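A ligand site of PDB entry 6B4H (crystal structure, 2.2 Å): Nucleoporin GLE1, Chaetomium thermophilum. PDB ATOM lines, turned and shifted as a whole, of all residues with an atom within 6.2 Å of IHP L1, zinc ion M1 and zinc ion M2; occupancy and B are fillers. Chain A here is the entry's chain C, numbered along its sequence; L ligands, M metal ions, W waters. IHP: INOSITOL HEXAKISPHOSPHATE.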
ATOM      1  N   HIS A  10      -4.878 -34.789   3.460  1.00  0.00           N
ATOM      2  CA  HIS A  10      -5.723 -34.025   2.549  1.00  0.00           C
ATOM      3  C   HIS A  10      -6.799 -34.908   1.915  1.00  0.00           C
ATOM      4  O   HIS A  10      -7.947 -34.484   1.756  1.00  0.00           O
ATOM      5  CB  HIS A  10      -4.852 -33.384   1.475  1.00  0.00           C
ATOM      6  CG  HIS A  10      -5.586 -32.436   0.572  1.00  0.00           C
ATOM      7  ND1 HIS A  10      -5.692 -32.630  -0.786  1.00  0.00           N
ATOM      8  CD2 HIS A  10      -6.229 -31.268   0.841  1.00  0.00           C
ATOM      9  CE1 HIS A  10      -6.383 -31.637  -1.310  1.00  0.00           C
ATOM     10  NE2 HIS A  10      -6.725 -30.798  -0.349  1.00  0.00           N
ATOM     11  N   LEU A  13      -9.457 -36.061   4.472  1.00  0.00           N
ATOM     12  CA  LEU A  13     -10.455 -35.013   4.698  1.00  0.00           C
ATOM     13  C   LEU A  13     -11.484 -34.977   3.580  1.00  0.00           C
ATOM     14  O   LEU A  13     -12.663 -34.728   3.832  1.00  0.00           O
ATOM     15  CB  LEU A  13      -9.754 -33.659   4.836  1.00  0.00           C
ATOM     16  CG  LEU A  13      -8.919 -33.476   6.107  1.00  0.00           C
ATOM     17  CD1 LEU A  13      -8.017 -32.255   5.976  1.00  0.00           C
ATOM     18  CD2 LEU A  13      -9.811 -33.363   7.333  1.00  0.00           C
ATOM     19  N   LYS A  14     -11.063 -35.219   2.329  1.00  0.00           N
ATOM     20  CA  LYS A  14     -12.022 -35.323   1.229  1.00  0.00           C
ATOM     21  C   LYS A  14     -13.045 -36.408   1.500  1.00  0.00           C
ATOM     22  O   LYS A  14     -14.253 -36.186   1.365  1.00  0.00           O
ATOM     23  CB  LYS A  14     -11.285 -35.627  -0.085  1.00  0.00           C
ATOM     24  CG  LYS A  14     -10.502 -34.476  -0.679  1.00  0.00           C
ATOM     25  CD  LYS A  14      -9.823 -34.911  -1.981  1.00  0.00           C
ATOM     26  CE  LYS A  14      -8.853 -33.847  -2.486  1.00  0.00           C
ATOM     27  NZ  LYS A  14      -9.555 -32.599  -2.870  1.00  0.00           N
ATOM     28  N   ARG A  17     -15.601 -35.496   4.238  1.00  0.00           N
ATOM     29  CA  ARG A  17     -16.681 -34.626   3.803  1.00  0.00           C
ATOM     30  C   ARG A  17     -17.727 -35.402   3.015  1.00  0.00           C
ATOM     31  O   ARG A  17     -18.932 -35.203   3.200  1.00  0.00           O
ATOM     32  CB  ARG A  17     -16.119 -33.458   2.974  1.00  0.00           C
ATOM     33  CG  ARG A  17     -15.186 -32.554   3.776  1.00  0.00           C
ATOM     34  CD  ARG A  17     -15.008 -31.170   3.140  1.00  0.00           C
ATOM     35  NE  ARG A  17     -14.437 -31.238   1.800  1.00  0.00           N
ATOM     36  CZ  ARG A  17     -13.145 -31.427   1.531  1.00  0.00           C
ATOM     37  NH1 ARG A  17     -12.276 -31.598   2.524  1.00  0.00           N
ATOM     38  NH2 ARG A  17     -12.727 -31.472   0.279  1.00  0.00           N
ATOM     39  N   LYS A  18     -17.294 -36.305   2.125  1.00  0.00           N
ATOM     40  CA  LYS A  18     -18.243 -37.166   1.438  1.00  0.00           C
ATOM     41  C   LYS A  18     -19.063 -37.994   2.432  1.00  0.00           C
ATOM     42  O   LYS A  18     -20.281 -38.132   2.281  1.00  0.00           O
ATOM     43  CB  LYS A  18     -17.520 -38.110   0.467  1.00  0.00           C
ATOM     44  CG  LYS A  18     -16.681 -37.416  -0.598  1.00  0.00           C
ATOM     45  CD  LYS A  18     -17.542 -36.686  -1.612  1.00  0.00           C
ATOM     46  CE  LYS A  18     -16.694 -36.112  -2.735  1.00  0.00           C
ATOM     47  NZ  LYS A  18     -17.497 -35.257  -3.650  1.00  0.00           N
ATOM     48  N   ARG A  38     -22.020 -25.333   9.069  1.00  0.00           N
ATOM     49  CA  ARG A  38     -21.062 -25.020   8.028  1.00  0.00           C
ATOM     50  C   ARG A  38     -21.184 -23.569   7.580  1.00  0.00           C
ATOM     51  O   ARG A  38     -20.198 -22.828   7.541  1.00  0.00           O
ATOM     52  CB  ARG A  38     -21.254 -25.967   6.838  1.00  0.00           C
ATOM     53  CG  ARG A  38     -20.365 -25.652   5.642  1.00  0.00           C
ATOM     54  CD  ARG A  38     -20.680 -26.549   4.456  1.00  0.00           C
ATOM     55  NE  ARG A  38     -19.946 -26.140   3.270  1.00  0.00           N
ATOM     56  CZ  ARG A  38     -20.309 -25.157   2.450  1.00  0.00           C
ATOM     57  NH1 ARG A  38     -21.429 -24.467   2.686  1.00  0.00           N
ATOM     58  NH2 ARG A  38     -19.569 -24.860   1.400  1.00  0.00           N
ATOM     59  N   ASN A 112     -12.256 -28.840   9.487  1.00  0.00           N
ATOM     60  CA  ASN A 112     -11.878 -28.811   8.084  1.00  0.00           C
ATOM     61  C   ASN A 112     -12.571 -27.677   7.341  1.00  0.00           C
ATOM     62  O   ASN A 112     -11.968 -27.010   6.504  1.00  0.00           O
ATOM     63  CB  ASN A 112     -12.190 -30.177   7.457  1.00  0.00           C
ATOM     64  CG  ASN A 112     -11.780 -30.285   6.002  1.00  0.00           C
ATOM     65  OD1 ASN A 112     -12.433 -30.981   5.218  1.00  0.00           O
ATOM     66  ND2 ASN A 112     -10.694 -29.627   5.622  1.00  0.00           N
ATOM     67  N   LYS A 116     -10.648 -24.653   5.608  1.00  0.00           N
ATOM     68  CA  LYS A 116     -10.913 -24.320   4.215  1.00  0.00           C
ATOM     69  C   LYS A 116     -11.367 -22.864   4.072  1.00  0.00           C
ATOM     70  O   LYS A 116     -10.960 -22.175   3.132  1.00  0.00           O
ATOM     71  CB  LYS A 116     -11.960 -25.270   3.640  1.00  0.00           C
ATOM     72  CG  LYS A 116     -11.395 -26.634   3.236  1.00  0.00           C
ATOM     73  CD  LYS A 116     -12.479 -27.716   3.130  1.00  0.00           C
ATOM     74  CE  LYS A 116     -13.515 -27.416   2.069  1.00  0.00           C
ATOM     75  NZ  LYS A 116     -12.951 -27.361   0.687  1.00  0.00           N
ATOM     76  N   ALA A 117     -12.187 -22.387   5.008  1.00  0.00           N
ATOM     77  CA  ALA A 117     -12.642 -20.998   4.931  1.00  0.00           C
ATOM     78  C   ALA A 117     -11.497 -20.041   5.160  1.00  0.00           C
ATOM     79  O   ALA A 117     -11.384 -19.017   4.463  1.00  0.00           O
ATOM     80  CB  ALA A 117     -13.762 -20.754   5.939  1.00  0.00           C
ATOM     81  N   ILE A 119      -8.293 -20.535   4.533  1.00  0.00           N
ATOM     82  CA  ILE A 119      -7.481 -20.552   3.310  1.00  0.00           C
ATOM     83  C   ILE A 119      -8.130 -19.704   2.227  1.00  0.00           C
ATOM     84  O   ILE A 119      -7.442 -18.983   1.494  1.00  0.00           O
ATOM     85  CB  ILE A 119      -7.257 -22.003   2.838  1.00  0.00           C
ATOM     86  CG1 ILE A 119      -6.328 -22.767   3.786  1.00  0.00           C
ATOM     87  CG2 ILE A 119      -6.725 -22.039   1.403  1.00  0.00           C
ATOM     88  CD1 ILE A 119      -4.886 -22.292   3.786  1.00  0.00           C
ATOM     89  N   SER A 120      -9.455 -19.784   2.107  1.00  0.00           N
ATOM     90  CA  SER A 120     -10.137 -19.043   1.051  1.00  0.00           C
ATOM     91  C   SER A 120     -10.052 -17.540   1.286  1.00  0.00           C
ATOM     92  O   SER A 120      -9.954 -16.762   0.338  1.00  0.00           O
ATOM     93  CB  SER A 120     -11.600 -19.477   0.946  1.00  0.00           C
ATOM     94  OG  SER A 120     -11.689 -20.774   0.371  1.00  0.00           O
ATOM     95  N   LYS A 163      -3.733 -28.512   3.841  1.00  0.00           N
ATOM     96  CA  LYS A 163      -4.263 -27.739   2.726  1.00  0.00           C
ATOM     97  C   LYS A 163      -3.260 -26.680   2.264  1.00  0.00           C
ATOM     98  O   LYS A 163      -3.118 -26.438   1.062  1.00  0.00           O
ATOM     99  CB  LYS A 163      -5.589 -27.095   3.110  1.00  0.00           C
ATOM    100  CG  LYS A 163      -6.249 -26.280   1.990  1.00  0.00           C
ATOM    101  CD  LYS A 163      -6.525 -27.126   0.753  1.00  0.00           C
ATOM    102  CE  LYS A 163      -7.224 -26.333  -0.338  1.00  0.00           C
ATOM    103  NZ  LYS A 163      -8.687 -26.154  -0.060  1.00  0.00           N
ATOM    104  N   ILE A 166      -0.968 -27.969  -0.215  1.00  0.00           N
ATOM    105  CA  ILE A 166      -1.529 -28.139  -1.547  1.00  0.00           C
ATOM    106  C   ILE A 166      -1.426 -26.844  -2.337  1.00  0.00           C
ATOM    107  O   ILE A 166      -1.047 -26.840  -3.511  1.00  0.00           O
ATOM    108  CB  ILE A 166      -2.995 -28.622  -1.451  1.00  0.00           C
ATOM    109  CG1 ILE A 166      -3.097 -29.980  -0.731  1.00  0.00           C
ATOM    110  CG2 ILE A 166      -3.622 -28.704  -2.840  1.00  0.00           C
ATOM    111  CD1 ILE A 166      -2.423 -31.138  -1.447  1.00  0.00           C
ATOM    112  N   VAL A 167      -1.781 -25.727  -1.710  1.00  0.00           N
ATOM    113  CA  VAL A 167      -1.994 -24.478  -2.443  1.00  0.00           C
ATOM    114  C   VAL A 167      -0.768 -23.578  -2.488  1.00  0.00           C
ATOM    115  O   VAL A 167      -0.712 -22.664  -3.326  1.00  0.00           O
ATOM    116  CB  VAL A 167      -3.175 -23.700  -1.853  1.00  0.00           C
ATOM    117  CG1 VAL A 167      -4.461 -24.513  -1.950  1.00  0.00           C
ATOM    118  CG2 VAL A 167      -2.887 -23.306  -0.412  1.00  0.00           C
ATOM    119  N   TRP A 190      -2.515 -22.840  -9.952  1.00  0.00           N
ATOM    120  CA  TRP A 190      -3.843 -23.418  -9.876  1.00  0.00           C
ATOM    121  C   TRP A 190      -4.513 -23.483 -11.255  1.00  0.00           C
ATOM    122  O   TRP A 190      -4.015 -22.947 -12.248  1.00  0.00           O
ATOM    123  CB  TRP A 190      -4.718 -22.627  -8.909  1.00  0.00           C
ATOM    124  CG  TRP A 190      -5.626 -23.497  -8.090  1.00  0.00           C
ATOM    125  CD1 TRP A 190      -6.987 -23.456  -8.054  1.00  0.00           C
ATOM    126  CD2 TRP A 190      -5.224 -24.555  -7.211  1.00  0.00           C
ATOM    127  NE1 TRP A 190      -7.457 -24.412  -7.188  1.00  0.00           N
ATOM    128  CE2 TRP A 190      -6.401 -25.102  -6.661  1.00  0.00           C
ATOM    129  CE3 TRP A 190      -3.985 -25.087  -6.825  1.00  0.00           C
ATOM    130  CZ2 TRP A 190      -6.374 -26.160  -5.748  1.00  0.00           C
ATOM    131  CZ3 TRP A 190      -3.964 -26.133  -5.921  1.00  0.00           C
ATOM    132  CH2 TRP A 190      -5.155 -26.655  -5.392  1.00  0.00           C
HETATM  133  C1  IHP L   1     -10.962 -29.236  -4.359  1.00  0.00           C
HETATM  134  C2  IHP L   1     -10.954 -28.385  -3.110  1.00  0.00           C
HETATM  135  C3  IHP L   1     -12.166 -27.463  -3.112  1.00  0.00           C
HETATM  136  C4  IHP L   1     -13.439 -28.281  -3.154  1.00  0.00           C
HETATM  137  C5  IHP L   1     -13.470 -29.181  -4.378  1.00  0.00           C
HETATM  138  C6  IHP L   1     -12.240 -30.057  -4.430  1.00  0.00           C
HETATM  139  O11 IHP L   1      -9.852 -30.155  -4.326  1.00  0.00           O
HETATM  140  P1  IHP L   1      -8.350 -29.804  -4.673  1.00  0.00           P
HETATM  141  O21 IHP L   1      -7.533 -31.030  -4.476  1.00  0.00           O
HETATM  142  O31 IHP L   1      -8.333 -29.299  -6.103  1.00  0.00           O
HETATM  143  O41 IHP L   1      -7.952 -28.669  -3.722  1.00  0.00           O
HETATM  144  O12 IHP L   1     -11.040 -29.246  -1.944  1.00  0.00           O
HETATM  145  P2  IHP L   1      -9.931 -29.509  -0.834  1.00  0.00           P
HETATM  146  O22 IHP L   1      -8.590 -29.137  -1.378  1.00  0.00           O
HETATM  147  O32 IHP L   1     -10.308 -28.692   0.413  1.00  0.00           O
HETATM  148  O42 IHP L   1     -10.035 -30.995  -0.474  1.00  0.00           O
HETATM  149  O13 IHP L   1     -12.173 -26.678  -1.907  1.00  0.00           O
HETATM  150  P3  IHP L   1     -11.641 -25.190  -1.760  1.00  0.00           P
HETATM  151  O23 IHP L   1     -10.223 -25.104  -2.206  1.00  0.00           O
HETATM  152  O33 IHP L   1     -11.821 -24.836  -0.284  1.00  0.00           O
HETATM  153  O43 IHP L   1     -12.547 -24.296  -2.589  1.00  0.00           O
HETATM  154  O14 IHP L   1     -14.544 -27.349  -3.253  1.00  0.00           O
HETATM  155  P4  IHP L   1     -15.510 -26.880  -2.101  1.00  0.00           P
HETATM  156  O24 IHP L   1     -15.383 -27.709  -0.882  1.00  0.00           O
HETATM  157  O34 IHP L   1     -15.172 -25.401  -1.870  1.00  0.00           O
HETATM  158  O44 IHP L   1     -16.915 -26.965  -2.715  1.00  0.00           O
HETATM  159  O15 IHP L   1     -14.619 -30.043  -4.254  1.00  0.00           O
HETATM  160  P5  IHP L   1     -15.847 -30.137  -5.227  1.00  0.00           P
HETATM  161  O25 IHP L   1     -16.364 -28.771  -5.543  1.00  0.00           O
HETATM  162  O35 IHP L   1     -16.898 -31.010  -4.519  1.00  0.00           O
HETATM  163  O45 IHP L   1     -15.322 -30.885  -6.453  1.00  0.00           O
HETATM  164  O16 IHP L   1     -12.246 -30.787  -5.678  1.00  0.00           O
HETATM  165  P6  IHP L   1     -12.157 -32.385  -5.746  1.00  0.00           P
HETATM  166  O26 IHP L   1     -11.791 -32.935  -4.433  1.00  0.00           O
HETATM  167  O36 IHP L   1     -13.535 -32.845  -6.209  1.00  0.00           O
HETATM  168  O46 IHP L   1     -11.119 -32.695  -6.823  1.00  0.00           O
HETATM  169  C1  IHP L   2     -19.345 -23.912  -4.800  1.00  0.00           C
HETATM  170  C2  IHP L   2     -20.473 -22.913  -4.890  1.00  0.00           C
HETATM  171  C3  IHP L   2     -20.482 -22.070  -3.631  1.00  0.00           C
HETATM  172  C4  IHP L   2     -19.168 -21.316  -3.497  1.00  0.00           C
HETATM  173  C5  IHP L   2     -18.032 -22.315  -3.402  1.00  0.00           C
HETATM  174  C6  IHP L   2     -18.015 -23.192  -4.649  1.00  0.00           C
HETATM  175  O11 IHP L   2     -19.323 -24.702  -6.011  1.00  0.00           O
HETATM  176  P1  IHP L   2     -19.772 -26.227  -6.078  1.00  0.00           P
HETATM  177  O21 IHP L   2     -19.111 -27.026  -5.000  1.00  0.00           O
HETATM  178  O31 IHP L   2     -19.373 -26.699  -7.474  1.00  0.00           O
HETATM  179  O41 IHP L   2     -21.287 -26.231  -5.977  1.00  0.00           O
HETATM  180  O12 IHP L   2     -20.228 -22.049  -6.025  1.00  0.00           O
HETATM  181  P2  IHP L   2     -21.050 -21.848  -7.381  1.00  0.00           P
HETATM  182  O22 IHP L   2     -20.374 -22.532  -8.535  1.00  0.00           O
HETATM  183  O32 IHP L   2     -22.463 -22.407  -7.116  1.00  0.00           O
HETATM  184  O42 IHP L   2     -21.158 -20.339  -7.574  1.00  0.00           O
HETATM  185  O13 IHP L   2     -21.585 -21.135  -3.676  1.00  0.00           O
HETATM  186  P3  IHP L   2     -22.904 -21.328  -2.809  1.00  0.00           P
HETATM  187  O23 IHP L   2     -23.727 -22.457  -3.346  1.00  0.00           O
HETATM  188  O33 IHP L   2     -23.629 -19.976  -2.848  1.00  0.00           O
HETATM  189  O43 IHP L   2     -22.423 -21.602  -1.373  1.00  0.00           O
HETATM  190  O14 IHP L   2     -19.215 -20.523  -2.285  1.00  0.00           O
HETATM  191  P4  IHP L   2     -19.054 -18.949  -2.160  1.00  0.00           P
HETATM  192  O24 IHP L   2     -17.600 -18.575  -2.205  1.00  0.00           O
HETATM  193  O34 IHP L   2     -19.724 -18.559  -0.849  1.00  0.00           O
HETATM  194  O44 IHP L   2     -19.853 -18.361  -3.313  1.00  0.00           O
HETATM  195  O15 IHP L   2     -16.776 -21.610  -3.302  1.00  0.00           O
HETATM  196  P5  IHP L   2     -15.858 -21.454  -2.009  1.00  0.00           P
HETATM  197  O25 IHP L   2     -15.475 -20.022  -1.826  1.00  0.00           O
HETATM  198  O35 IHP L   2     -14.658 -22.372  -2.215  1.00  0.00           O
HETATM  199  O45 IHP L   2     -16.664 -21.997  -0.845  1.00  0.00           O
HETATM  200  O16 IHP L   2     -16.975 -24.172  -4.499  1.00  0.00           O
HETATM  201  P6  IHP L   2     -15.879 -24.481  -5.593  1.00  0.00           P
HETATM  202  O26 IHP L   2     -16.080 -23.627  -6.790  1.00  0.00           O
HETATM  203  O36 IHP L   2     -16.035 -25.978  -5.904  1.00  0.00           O
HETATM  204  O46 IHP L   2     -14.533 -24.231  -4.902  1.00  0.00           O
HETATM  205 ZN    ZN M   1     -14.380 -24.165  -2.922  1.00  0.00          ZN
HETATM  206 ZN    ZN M   2     -17.020 -27.287  -4.647  1.00  0.00          ZN
HETATM  207  O   HOH W   1      -9.864 -30.269  -8.001  1.00  0.00           O
HETATM  208  O   HOH W   2     -17.105 -28.155   1.472  1.00  0.00           O
HETATM  209  O   HOH W   3      -9.183 -32.117   1.907  1.00  0.00           O
HETATM  210  O   HOH W   4     -15.427 -30.710  -1.009  1.00  0.00           O
HETATM  211  O   HOH W   5      -9.247 -29.533   3.011  1.00  0.00           O
HETATM  212  O   HOH W   6      -9.609 -25.187  -4.787  1.00  0.00           O
HETATM  213  O   HOH W   7      -9.658 -23.686   0.998  1.00  0.00           O
HETATM  214  O   HOH W   8      -9.513 -27.017  -6.827  1.00  0.00           O
HETATM  215  O   HOH W   9     -18.890 -25.520  -1.520  1.00  0.00           O
HETATM  216  O   HOH W  10      -8.995 -22.539  -1.447  1.00  0.00           O
HETATM  217  O   HOH W  11     -13.272 -22.623   0.285  1.00  0.00           O
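No residue comes within 4 Å of zinc ion M1.
Zinc ion M1 is bound by O34 of IHP L1, O43 of IHP L1, O35 of IHP L2 and O46 of IHP L2.
O22 of IHP L1 sits at hydrogen-bond distance from NE2 of His 10, at 2.7 Å. The side-chain amino group (NZ) of Lys 14 is in salt-bridge range of an oxygen (O26) of IHP L1, at 2.7 Å. The side-chain amino group of Lys 116 lies within salt-bridge range of an oxygen (O24) of IHP L1, 2.9 Å away. An oxygen (O42) of IHP L1 is in salt-bridge range of the guanidinium group (NH2) of Arg 17. The side-chain amino group (NZ) of Lys 163 lies within salt-bridge range of an oxygen (O23) of IHP L1.
Zinc ion M2 is bound by an oxygen (O25) of IHP L1 (1.9 Å), an oxygen (O44) of IHP L1 (2.0 Å), an oxygen (O36) of IHP L2 (2.1 Å) and an oxygen (O21) of IHP L2 (2.1 Å). Slightly farther from zinc ion M2 lies O14 of IHP L1 (2.8 Å).
Water W8 bridges O31 of IHP L1 (2.7 Å) and NE1 of Trp 190 (3.3 Å). Water W11 bridges the side-chain hydroxyl (OG) of Ser 120 (2.4 Å) and an oxygen (O33) of IHP L1 (2.7 Å). Water W7 lies within hydrogen-bond range of an oxygen (O33) of IHP L1 (2.8 Å), the side-chain amino group of Lys 163 (2.9 Å) and the backbone carbonyl oxygen of Lys 116 (2.9 Å). Water W3 lies within hydrogen-bond range of O of His 10 (2.7 Å), O42 of IHP L1 (2.8 Å) and NH1 of Arg 17 (3.2 Å). Water W5 bridges O32 of IHP L1 and ND2 of Asn 112. Water W4 lies within hydrogen-bond range of O24 of IHP L1 and NE of Arg 17.
CZ2 of Trp 190 touches O41 of IHP L1 (3.6 Å). Hydrophobic or aromatic side chains that line IHP L1: His 10 and Trp 190. Within 4 Å of IHP L1: His 10, Lys 14, Arg 17, Lys 116, Lys 163 and Trp 190.
The side-chain hydroxyl (OG) of Ser 120 lies within hydrogen-bond range of the backbone carbonyl oxygen (O) of Lys 116 (3.2 Å). OD1 of Asn 112 lies within hydrogen-bond range of NH1 of Arg 17 (2.8 Å). The guanidinium group (NH1) of Arg 17 lies close to the backbone carbonyl oxygen (O) of Leu 13, 3.4 Å away.
No residue comes within 4 Å of zinc ion M2.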
